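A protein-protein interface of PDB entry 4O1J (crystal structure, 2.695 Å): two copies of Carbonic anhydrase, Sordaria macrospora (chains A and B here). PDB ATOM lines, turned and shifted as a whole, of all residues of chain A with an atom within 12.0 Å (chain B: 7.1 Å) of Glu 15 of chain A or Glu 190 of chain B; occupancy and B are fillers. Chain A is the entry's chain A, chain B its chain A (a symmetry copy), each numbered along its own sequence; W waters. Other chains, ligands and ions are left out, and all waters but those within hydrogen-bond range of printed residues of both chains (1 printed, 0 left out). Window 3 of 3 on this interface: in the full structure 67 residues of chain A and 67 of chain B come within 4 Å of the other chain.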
ATOM      1  N   GLU A  15      30.141  21.261 -25.028  1.00  0.00           N
ATOM      2  CA  GLU A  15      29.239  20.115 -24.962  1.00  0.00           C
ATOM      3  C   GLU A  15      27.800  20.592 -24.835  1.00  0.00           C
ATOM      4  O   GLU A  15      26.858  19.819 -24.989  1.00  0.00           O
ATOM      5  CB  GLU A  15      29.611  19.201 -23.789  1.00  0.00           C
ATOM      6  CG  GLU A  15      29.465  17.715 -24.086  1.00  0.00           C
ATOM      7  CD  GLU A  15      30.091  16.836 -23.015  1.00  0.00           C
ATOM      8  OE1 GLU A  15      30.963  17.332 -22.264  1.00  0.00           O
ATOM      9  OE2 GLU A  15      29.705  15.646 -22.923  1.00  0.00           O
ATOM     10  N   ASN A  16      27.662  21.888 -24.578  1.00  0.00           N
ATOM     11  CA  ASN A  16      26.393  22.531 -24.268  1.00  0.00           C
ATOM     12  C   ASN A  16      25.256  22.218 -25.244  1.00  0.00           C
ATOM     13  O   ASN A  16      24.191  21.782 -24.818  1.00  0.00           O
ATOM     14  CB  ASN A  16      26.599  24.045 -24.169  1.00  0.00           C
ATOM     15  CG  ASN A  16      25.368  24.769 -23.645  1.00  0.00           C
ATOM     16  OD1 ASN A  16      24.588  24.211 -22.862  1.00  0.00           O
ATOM     17  ND2 ASN A  16      25.207  26.030 -24.046  1.00  0.00           N
ATOM     18  N   THR A  17      25.475  22.437 -26.539  1.00  0.00           N
ATOM     19  CA  THR A  17      24.441  22.193 -27.555  1.00  0.00           C
ATOM     20  C   THR A  17      24.037  20.722 -27.703  1.00  0.00           C
ATOM     21  O   THR A  17      22.868  20.403 -27.971  1.00  0.00           O
ATOM     22  CB  THR A  17      24.910  22.682 -28.939  1.00  0.00           C
ATOM     23  OG1 THR A  17      25.516  23.976 -28.818  1.00  0.00           O
ATOM     24  CG2 THR A  17      23.741  22.747 -29.909  1.00  0.00           C
ATOM     25  N   PHE A  18      24.996  19.828 -27.509  1.00  0.00           N
ATOM     26  CA  PHE A  18      24.712  18.402 -27.499  1.00  0.00           C
ATOM     27  C   PHE A  18      23.837  18.013 -26.298  1.00  0.00           C
ATOM     28  O   PHE A  18      22.870  17.244 -26.424  1.00  0.00           O
ATOM     29  CB  PHE A  18      26.025  17.622 -27.508  1.00  0.00           C
ATOM     30  CG  PHE A  18      25.876  16.174 -27.169  1.00  0.00           C
ATOM     31  CD1 PHE A  18      26.353  15.683 -25.966  1.00  0.00           C
ATOM     32  CD2 PHE A  18      25.284  15.299 -28.061  1.00  0.00           C
ATOM     33  CE1 PHE A  18      26.231  14.345 -25.655  1.00  0.00           C
ATOM     34  CE2 PHE A  18      25.157  13.960 -27.755  1.00  0.00           C
ATOM     35  CZ  PHE A  18      25.629  13.482 -26.553  1.00  0.00           C
ATOM     36  N   HIS A  19      24.167  18.561 -25.133  1.00  0.00           N
ATOM     37  CA  HIS A  19      23.418  18.255 -23.919  1.00  0.00           C
ATOM     38  C   HIS A  19      22.024  18.873 -23.996  1.00  0.00           C
ATOM     39  O   HIS A  19      21.049  18.313 -23.477  1.00  0.00           O
ATOM     40  CB  HIS A  19      24.168  18.747 -22.680  1.00  0.00           C
ATOM     41  CG  HIS A  19      25.360  17.911 -22.322  1.00  0.00           C
ATOM     42  ND1 HIS A  19      25.339  16.528 -22.345  1.00  0.00           N
ATOM     43  CD2 HIS A  19      26.614  18.256 -21.950  1.00  0.00           C
ATOM     44  CE1 HIS A  19      26.521  16.065 -21.993  1.00  0.00           C
ATOM     45  NE2 HIS A  19      27.316  17.094 -21.743  1.00  0.00           N
ATOM     46  N   TYR A  20      21.925  20.006 -24.686  1.00  0.00           N
ATOM     47  CA  TYR A  20      20.630  20.615 -24.937  1.00  0.00           C
ATOM     48  C   TYR A  20      19.820  19.701 -25.850  1.00  0.00           C
ATOM     49  O   TYR A  20      18.606  19.571 -25.685  1.00  0.00           O
ATOM     50  CB  TYR A  20      20.765  22.003 -25.566  1.00  0.00           C
ATOM     51  CG  TYR A  20      19.426  22.585 -25.973  1.00  0.00           C
ATOM     52  CD1 TYR A  20      18.524  23.042 -25.016  1.00  0.00           C
ATOM     53  CD2 TYR A  20      19.042  22.631 -27.310  1.00  0.00           C
ATOM     54  CE1 TYR A  20      17.287  23.554 -25.383  1.00  0.00           C
ATOM     55  CE2 TYR A  20      17.810  23.139 -27.684  1.00  0.00           C
ATOM     56  CZ  TYR A  20      16.935  23.600 -26.717  1.00  0.00           C
ATOM     57  OH  TYR A  20      15.707  24.104 -27.091  1.00  0.00           O
ATOM     58  N   ALA A  21      20.493  19.068 -26.812  1.00  0.00           N
ATOM     59  CA  ALA A  21      19.810  18.137 -27.718  1.00  0.00           C
ATOM     60  C   ALA A  21      19.263  16.915 -26.968  1.00  0.00           C
ATOM     61  O   ALA A  21      18.166  16.422 -27.267  1.00  0.00           O
ATOM     62  CB  ALA A  21      20.751  17.694 -28.837  1.00  0.00           C
ATOM     63  N   LEU A  22      20.022  16.438 -25.982  1.00  0.00           N
ATOM     64  CA  LEU A  22      19.553  15.327 -25.154  1.00  0.00           C
ATOM     65  C   LEU A  22      18.358  15.753 -24.303  1.00  0.00           C
ATOM     66  O   LEU A  22      17.371  15.016 -24.157  1.00  0.00           O
ATOM     67  CB  LEU A  22      20.684  14.802 -24.270  1.00  0.00           C
ATOM     68  CG  LEU A  22      21.840  14.161 -25.046  1.00  0.00           C
ATOM     69  CD1 LEU A  22      22.821  13.472 -24.107  1.00  0.00           C
ATOM     70  CD2 LEU A  22      21.318  13.187 -26.100  1.00  0.00           C
ATOM     71  N   SER A  23      18.459  16.951 -23.738  1.00  0.00           N
ATOM     72  CA  SER A  23      17.378  17.522 -22.946  1.00  0.00           C
ATOM     73  C   SER A  23      16.075  17.669 -23.749  1.00  0.00           C
ATOM     74  O   SER A  23      14.988  17.304 -23.275  1.00  0.00           O
ATOM     75  CB  SER A  23      17.817  18.880 -22.398  1.00  0.00           C
ATOM     76  OG  SER A  23      16.707  19.653 -21.995  1.00  0.00           O
ATOM     77  N   SER A  24      16.197  18.185 -24.970  1.00  0.00           N
ATOM     78  CA  SER A  24      15.045  18.412 -25.833  1.00  0.00           C
ATOM     79  C   SER A  24      14.473  17.085 -26.279  1.00  0.00           C
ATOM     80  O   SER A  24      13.267  16.954 -26.488  1.00  0.00           O
ATOM     81  CB  SER A  24      15.420  19.258 -27.050  1.00  0.00           C
ATOM     82  OG  SER A  24      15.906  20.528 -26.666  1.00  0.00           O
ATOM     83  N   VAL B 104      30.950  22.076 -37.743  1.00  0.00           N
ATOM     84  CA  VAL B 104      30.084  21.571 -36.680  1.00  0.00           C
ATOM     85  C   VAL B 104      30.913  21.299 -35.440  1.00  0.00           C
ATOM     86  O   VAL B 104      32.098  20.992 -35.524  1.00  0.00           O
ATOM     87  CB  VAL B 104      29.336  20.283 -37.080  1.00  0.00           C
ATOM     88  CG1 VAL B 104      28.359  20.556 -38.208  1.00  0.00           C
ATOM     89  CG2 VAL B 104      30.316  19.189 -37.456  1.00  0.00           C
ATOM     90  N   LYS B 105      30.287  21.429 -34.282  1.00  0.00           N
ATOM     91  CA  LYS B 105      31.010  21.324 -33.026  1.00  0.00           C
ATOM     92  C   LYS B 105      30.813  19.962 -32.368  1.00  0.00           C
ATOM     93  O   LYS B 105      31.553  19.598 -31.454  1.00  0.00           O
ATOM     94  CB  LYS B 105      30.571  22.449 -32.090  1.00  0.00           C
ATOM     95  CG  LYS B 105      30.686  23.818 -32.744  1.00  0.00           C
ATOM     96  CD  LYS B 105      29.988  24.900 -31.949  1.00  0.00           C
ATOM     97  CE  LYS B 105      29.967  26.199 -32.730  1.00  0.00           C
ATOM     98  NZ  LYS B 105      29.155  27.237 -32.038  1.00  0.00           N
ATOM     99  N   HIS B 106      29.818  19.216 -32.848  1.00  0.00           N
ATOM    100  CA  HIS B 106      29.483  17.906 -32.295  1.00  0.00           C
ATOM    101  C   HIS B 106      29.210  16.880 -33.385  1.00  0.00           C
ATOM    102  O   HIS B 106      28.543  17.180 -34.371  1.00  0.00           O
ATOM    103  CB  HIS B 106      28.258  18.012 -31.391  1.00  0.00           C
ATOM    104  CG  HIS B 106      28.461  18.911 -30.216  1.00  0.00           C
ATOM    105  ND1 HIS B 106      29.138  18.513 -29.086  1.00  0.00           N
ATOM    106  CD2 HIS B 106      28.113  20.203 -30.013  1.00  0.00           C
ATOM    107  CE1 HIS B 106      29.180  19.515 -28.227  1.00  0.00           C
ATOM    108  NE2 HIS B 106      28.566  20.553 -28.766  1.00  0.00           N
ATOM    109  N   ILE B 107      29.722  15.669 -33.190  1.00  0.00           N
ATOM    110  CA  ILE B 107      29.413  14.538 -34.055  1.00  0.00           C
ATOM    111  C   ILE B 107      28.751  13.459 -33.223  1.00  0.00           C
ATOM    112  O   ILE B 107      29.336  12.944 -32.283  1.00  0.00           O
ATOM    113  CB  ILE B 107      30.677  13.970 -34.758  1.00  0.00           C
ATOM    114  CG1 ILE B 107      31.252  15.008 -35.726  1.00  0.00           C
ATOM    115  CG2 ILE B 107      30.353  12.679 -35.503  1.00  0.00           C
ATOM    116  CD1 ILE B 107      32.565  14.625 -36.324  1.00  0.00           C
ATOM    117  N   VAL B 108      27.520  13.127 -33.582  1.00  0.00           N
ATOM    118  CA  VAL B 108      26.703  12.187 -32.835  1.00  0.00           C
ATOM    119  C   VAL B 108      26.472  10.904 -33.616  1.00  0.00           C
ATOM    120  O   VAL B 108      25.732  10.889 -34.603  1.00  0.00           O
ATOM    121  CB  VAL B 108      25.328  12.794 -32.479  1.00  0.00           C
ATOM    122  CG1 VAL B 108      24.511  11.811 -31.664  1.00  0.00           C
ATOM    123  CG2 VAL B 108      25.501  14.105 -31.734  1.00  0.00           C
ATOM    124  N   MET B 175      37.046   8.417 -34.601  1.00  0.00           N
ATOM    125  CA  MET B 175      38.133   8.975 -33.815  1.00  0.00           C
ATOM    126  C   MET B 175      39.464   8.748 -34.510  1.00  0.00           C
ATOM    127  O   MET B 175      40.463   9.384 -34.170  1.00  0.00           O
ATOM    128  CB  MET B 175      38.161   8.357 -32.414  1.00  0.00           C
ATOM    129  CG  MET B 175      36.905   8.609 -31.583  1.00  0.00           C
ATOM    130  SD  MET B 175      36.796  10.267 -30.889  1.00  0.00           S
ATOM    131  CE  MET B 175      37.955  10.147 -29.524  1.00  0.00           C
ATOM    132  N   ILE B 180      38.482  14.588 -38.434  1.00  0.00           N
ATOM    133  CA  ILE B 180      37.862  14.623 -37.123  1.00  0.00           C
ATOM    134  C   ILE B 180      38.951  14.800 -36.091  1.00  0.00           C
ATOM    135  O   ILE B 180      38.822  15.606 -35.179  1.00  0.00           O
ATOM    136  CB  ILE B 180      37.051  13.338 -36.849  1.00  0.00           C
ATOM    137  CG1 ILE B 180      35.762  13.349 -37.681  1.00  0.00           C
ATOM    138  CG2 ILE B 180      36.724  13.208 -35.375  1.00  0.00           C
ATOM    139  CD1 ILE B 180      34.945  12.091 -37.573  1.00  0.00           C
ATOM    140  N   ALA B 183      40.381  18.313 -36.187  1.00  0.00           N
ATOM    141  CA  ALA B 183      39.408  19.257 -35.658  1.00  0.00           C
ATOM    142  C   ALA B 183      39.296  19.131 -34.138  1.00  0.00           C
ATOM    143  O   ALA B 183      39.013  20.109 -33.444  1.00  0.00           O
ATOM    144  CB  ALA B 183      38.063  19.050 -36.313  1.00  0.00           C
ATOM    145  N   ILE B 184      39.532  17.929 -33.620  1.00  0.00           N
ATOM    146  CA  ILE B 184      39.569  17.731 -32.179  1.00  0.00           C
ATOM    147  C   ILE B 184      40.794  18.440 -31.629  1.00  0.00           C
ATOM    148  O   ILE B 184      40.719  19.153 -30.621  1.00  0.00           O
ATOM    149  CB  ILE B 184      39.630  16.243 -31.795  1.00  0.00           C
ATOM    150  CG1 ILE B 184      38.366  15.523 -32.254  1.00  0.00           C
ATOM    151  CG2 ILE B 184      39.781  16.094 -30.293  1.00  0.00           C
ATOM    152  CD1 ILE B 184      38.391  14.035 -32.029  1.00  0.00           C
ATOM    153  N   ARG B 187      40.191  22.636 -32.704  1.00  0.00           N
ATOM    154  CA  ARG B 187      38.913  23.328 -32.494  1.00  0.00           C
ATOM    155  C   ARG B 187      38.128  22.793 -31.305  1.00  0.00           C
ATOM    156  O   ARG B 187      37.111  23.365 -30.923  1.00  0.00           O
ATOM    157  CB  ARG B 187      38.001  23.211 -33.715  1.00  0.00           C
ATOM    158  CG  ARG B 187      38.314  24.082 -34.897  1.00  0.00           C
ATOM    159  CD  ARG B 187      37.368  23.694 -36.010  1.00  0.00           C
ATOM    160  NE  ARG B 187      36.136  23.158 -35.439  1.00  0.00           N
ATOM    161  CZ  ARG B 187      35.260  22.410 -36.098  1.00  0.00           C
ATOM    162  NH1 ARG B 187      35.472  22.104 -37.371  1.00  0.00           N
ATOM    163  NH2 ARG B 187      34.170  21.972 -35.482  1.00  0.00           N
ATOM    164  N   GLY B 188      38.564  21.666 -30.760  1.00  0.00           N
ATOM    165  CA  GLY B 188      37.836  21.036 -29.682  1.00  0.00           C
ATOM    166  C   GLY B 188      36.540  20.440 -30.187  1.00  0.00           C
ATOM    167  O   GLY B 188      35.504  20.523 -29.524  1.00  0.00           O
ATOM    168  N   LEU B 189      36.599  19.843 -31.371  1.00  0.00           N
ATOM    169  CA  LEU B 189      35.461  19.120 -31.907  1.00  0.00           C
ATOM    170  C   LEU B 189      35.135  17.980 -30.954  1.00  0.00           C
ATOM    171  O   LEU B 189      36.036  17.322 -30.424  1.00  0.00           O
ATOM    172  CB  LEU B 189      35.754  18.604 -33.322  1.00  0.00           C
ATOM    173  CG  LEU B 189      34.728  17.646 -33.937  1.00  0.00           C
ATOM    174  CD1 LEU B 189      33.361  18.302 -33.998  1.00  0.00           C
ATOM    175  CD2 LEU B 189      35.162  17.222 -35.322  1.00  0.00           C
ATOM    176  N   GLU B 190      33.852  17.765 -30.701  1.00  0.00           N
ATOM    177  CA  GLU B 190      33.457  16.697 -29.795  1.00  0.00           C
ATOM    178  C   GLU B 190      32.749  15.571 -30.529  1.00  0.00           C
ATOM    179  O   GLU B 190      32.056  15.801 -31.516  1.00  0.00           O
ATOM    180  CB  GLU B 190      32.578  17.244 -28.672  1.00  0.00           C
ATOM    181  CG  GLU B 190      33.320  18.201 -27.752  1.00  0.00           C
ATOM    182  CD  GLU B 190      32.543  18.521 -26.491  1.00  0.00           C
ATOM    183  OE1 GLU B 190      32.181  17.575 -25.761  1.00  0.00           O
ATOM    184  OE2 GLU B 190      32.302  19.720 -26.229  1.00  0.00           O
ATOM    185  N   VAL B 191      32.960  14.347 -30.055  1.00  0.00           N
ATOM    186  CA  VAL B 191      32.344  13.178 -30.661  1.00  0.00           C
ATOM    187  C   VAL B 191      31.651  12.347 -29.580  1.00  0.00           C
ATOM    188  O   VAL B 191      32.222  12.080 -28.524  1.00  0.00           O
ATOM    189  CB  VAL B 191      33.379  12.317 -31.412  1.00  0.00           C
ATOM    190  CG1 VAL B 191      32.691  11.149 -32.119  1.00  0.00           C
ATOM    191  CG2 VAL B 191      34.148  13.174 -32.414  1.00  0.00           C
ATOM    192  N   HIS B 192      30.413  11.949 -29.850  1.00  0.00           N
ATOM    193  CA  HIS B 192      29.575  11.274 -28.869  1.00  0.00           C
ATOM    194  C   HIS B 192      28.932  10.022 -29.457  1.00  0.00           C
ATOM    195  O   HIS B 192      28.419  10.036 -30.583  1.00  0.00           O
ATOM    196  CB  HIS B 192      28.492  12.226 -28.350  1.00  0.00           C
ATOM    197  CG  HIS B 192      28.973  13.629 -28.148  1.00  0.00           C
ATOM    198  ND1 HIS B 192      29.602  14.044 -26.993  1.00  0.00           N
ATOM    199  CD2 HIS B 192      28.938  14.712 -28.967  1.00  0.00           C
ATOM    200  CE1 HIS B 192      29.926  15.320 -27.102  1.00  0.00           C
ATOM    201  NE2 HIS B 192      29.534  15.747 -28.292  1.00  0.00           N
ATOM    202  N   GLU B 205      23.666   8.304 -23.460  1.00  0.00           N
ATOM    203  CA  GLU B 205      25.063   8.254 -23.871  1.00  0.00           C
ATOM    204  C   GLU B 205      25.634   6.871 -23.600  1.00  0.00           C
ATOM    205  O   GLU B 205      25.327   6.267 -22.580  1.00  0.00           O
ATOM    206  CB  GLU B 205      25.882   9.317 -23.145  1.00  0.00           C
ATOM    207  CG  GLU B 205      25.415  10.727 -23.398  1.00  0.00           C
ATOM    208  CD  GLU B 205      26.230  11.744 -22.630  1.00  0.00           C
ATOM    209  OE1 GLU B 205      27.476  11.644 -22.651  1.00  0.00           O
ATOM    210  OE2 GLU B 205      25.628  12.653 -22.018  1.00  0.00           O
ATOM    211  N   GLY B 209      33.583   8.129 -26.935  1.00  0.00           N
ATOM    212  CA  GLY B 209      33.750   9.332 -27.721  1.00  0.00           C
ATOM    213  C   GLY B 209      34.898  10.176 -27.221  1.00  0.00           C
ATOM    214  O   GLY B 209      35.833   9.674 -26.596  1.00  0.00           O
ATOM    215  N   THR B 210      34.812  11.471 -27.494  1.00  0.00           N
ATOM    216  CA  THR B 210      35.875  12.408 -27.167  1.00  0.00           C
ATOM    217  C   THR B 210      36.084  12.613 -25.654  1.00  0.00           C
ATOM    218  O   THR B 210      37.218  12.792 -25.210  1.00  0.00           O
ATOM    219  CB  THR B 210      35.632  13.761 -27.885  1.00  0.00           C
ATOM    220  OG1 THR B 210      36.870  14.473 -27.999  1.00  0.00           O
ATOM    221  CG2 THR B 210      34.593  14.606 -27.168  1.00  0.00           C
ATOM    222  N   ALA B 211      35.010  12.571 -24.871  1.00  0.00           N
ATOM    223  CA  ALA B 211      35.100  12.791 -23.426  1.00  0.00           C
ATOM    224  C   ALA B 211      33.771  12.502 -22.740  1.00  0.00           C
ATOM    225  O   ALA B 211      33.350  13.238 -21.848  1.00  0.00           O
ATOM    226  CB  ALA B 211      35.547  14.224 -23.122  1.00  0.00           C
HETATM  227  O   HOH W   1      28.777  23.239 -27.574  1.00  0.00           O
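Printed residues of chain B within 4 Å of Glu 15 of chain A: His 106, Glu 190 and His 192.
Printed residues of chain A within 4 Å of His 106 of chain B: Glu 15 and Phe 18.
No residue of chain A comes within 4 Å of Ile 107 of chain B.
No residue of chain A comes within 4 Å of Leu 189 of chain B.
No residue of chain A comes within 4 Å of Val 191 of chain B.
No residue of chain A comes within 4 Å of Thr 210 of chain B.
No residue of chain A comes within 4 Å of Ala 211 of chain B.
Of the printed residues of chain A, Glu 205 of chain B touches Phe 18, His 19 and Leu 22.
Of the printed residues of chain B, His 19 of chain A touches Glu 205 (3.5 Å).
Of the printed residues of chain B, Phe 18 of chain A touches His 106, Val 108, His 192 and Glu 205.
Of the printed residues of chain A, Val 108 of chain B touches Phe 18 (3.9 Å).
Asn 16 of chain A touches none of the printed residues of chain B.
Thr 17 of chain A touches none of the printed residues of chain B.
The nearest residue of chain B that does not touch Glu 15 of chain A is Ala 211 of chain B (4.5 Å).
The nearest residue of chain A that does not touch Glu 190 of chain B is Asn 16 of chain A (5.4 Å).
The nearest printed residue of chain B that does not touch His 19 of chain A is His 106 of chain B (6.0 Å).
The backbone NH (N) of Ile 107 of chain B lies within hydrogen-bond range of the backbone carbonyl oxygen (O) of Glu 190 of chain B (2.9 Å).
A ring nitrogen (ND1) of His 106 of chain B sits at hydrogen-bond distance from a ring nitrogen (NE2) of His 192 of chain B.
N of Glu 190 of chain B is in hydrogen-bond range of O of Lys 105 of chain B (3.0 Å).
A ring nitrogen (NE2) of His 19 of chain A lies within hydrogen-bond range of the side-chain carboxylate (OE2) of Glu 15 of chain A (3.0 Å).
O of Ile 107 of chain B lies within hydrogen-bond range of N of His 192 of chain B (2.8 Å).
Among the printed residues, merely in contact across the chains: Glu 15 of chain A with His 106 of chain B, His 19 of chain A with Glu 205 of chain B, Leu 22 of chain A with Glu 205 of chain B, Phe 18 of chain A with His 106 of chain B, Phe 18 of chain A with His 192 of chain B, Phe 18 of chain A with Val 108 of chain B, Glu 15 of chain A with His 192 of chain B and Phe 18 of chain A with Glu 205 of chain B.
The side-chain carboxylate (OE2) of Glu 190 of chain B lies within hydrogen-bond range of the backbone NH (N) of Glu 15 of chain A.
No position is printed for both chains.
Hydrophobic or aromatic side chains of chain A within 4 Å of the printed part of chain B: Phe 18, His 19 and Leu 22.
Along chain A the printed residues that touch a printed residue of chain B span positions 15 to 22.
Of the 19 printed residues of chain B, 5 touch a printed residue of chain A.
Printed residues of chain B that touch a printed residue of chain A: His 106, Val 108, Glu 190, His 192 and Glu 205.
Among the printed residues, 9 pairs touch across the chains.
Water W1 bridges a ring nitrogen (NE2) of His 106 of chain B (2.9 Å) and the backbone NH (N) of Asn 16 of chain A (3.5 Å).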
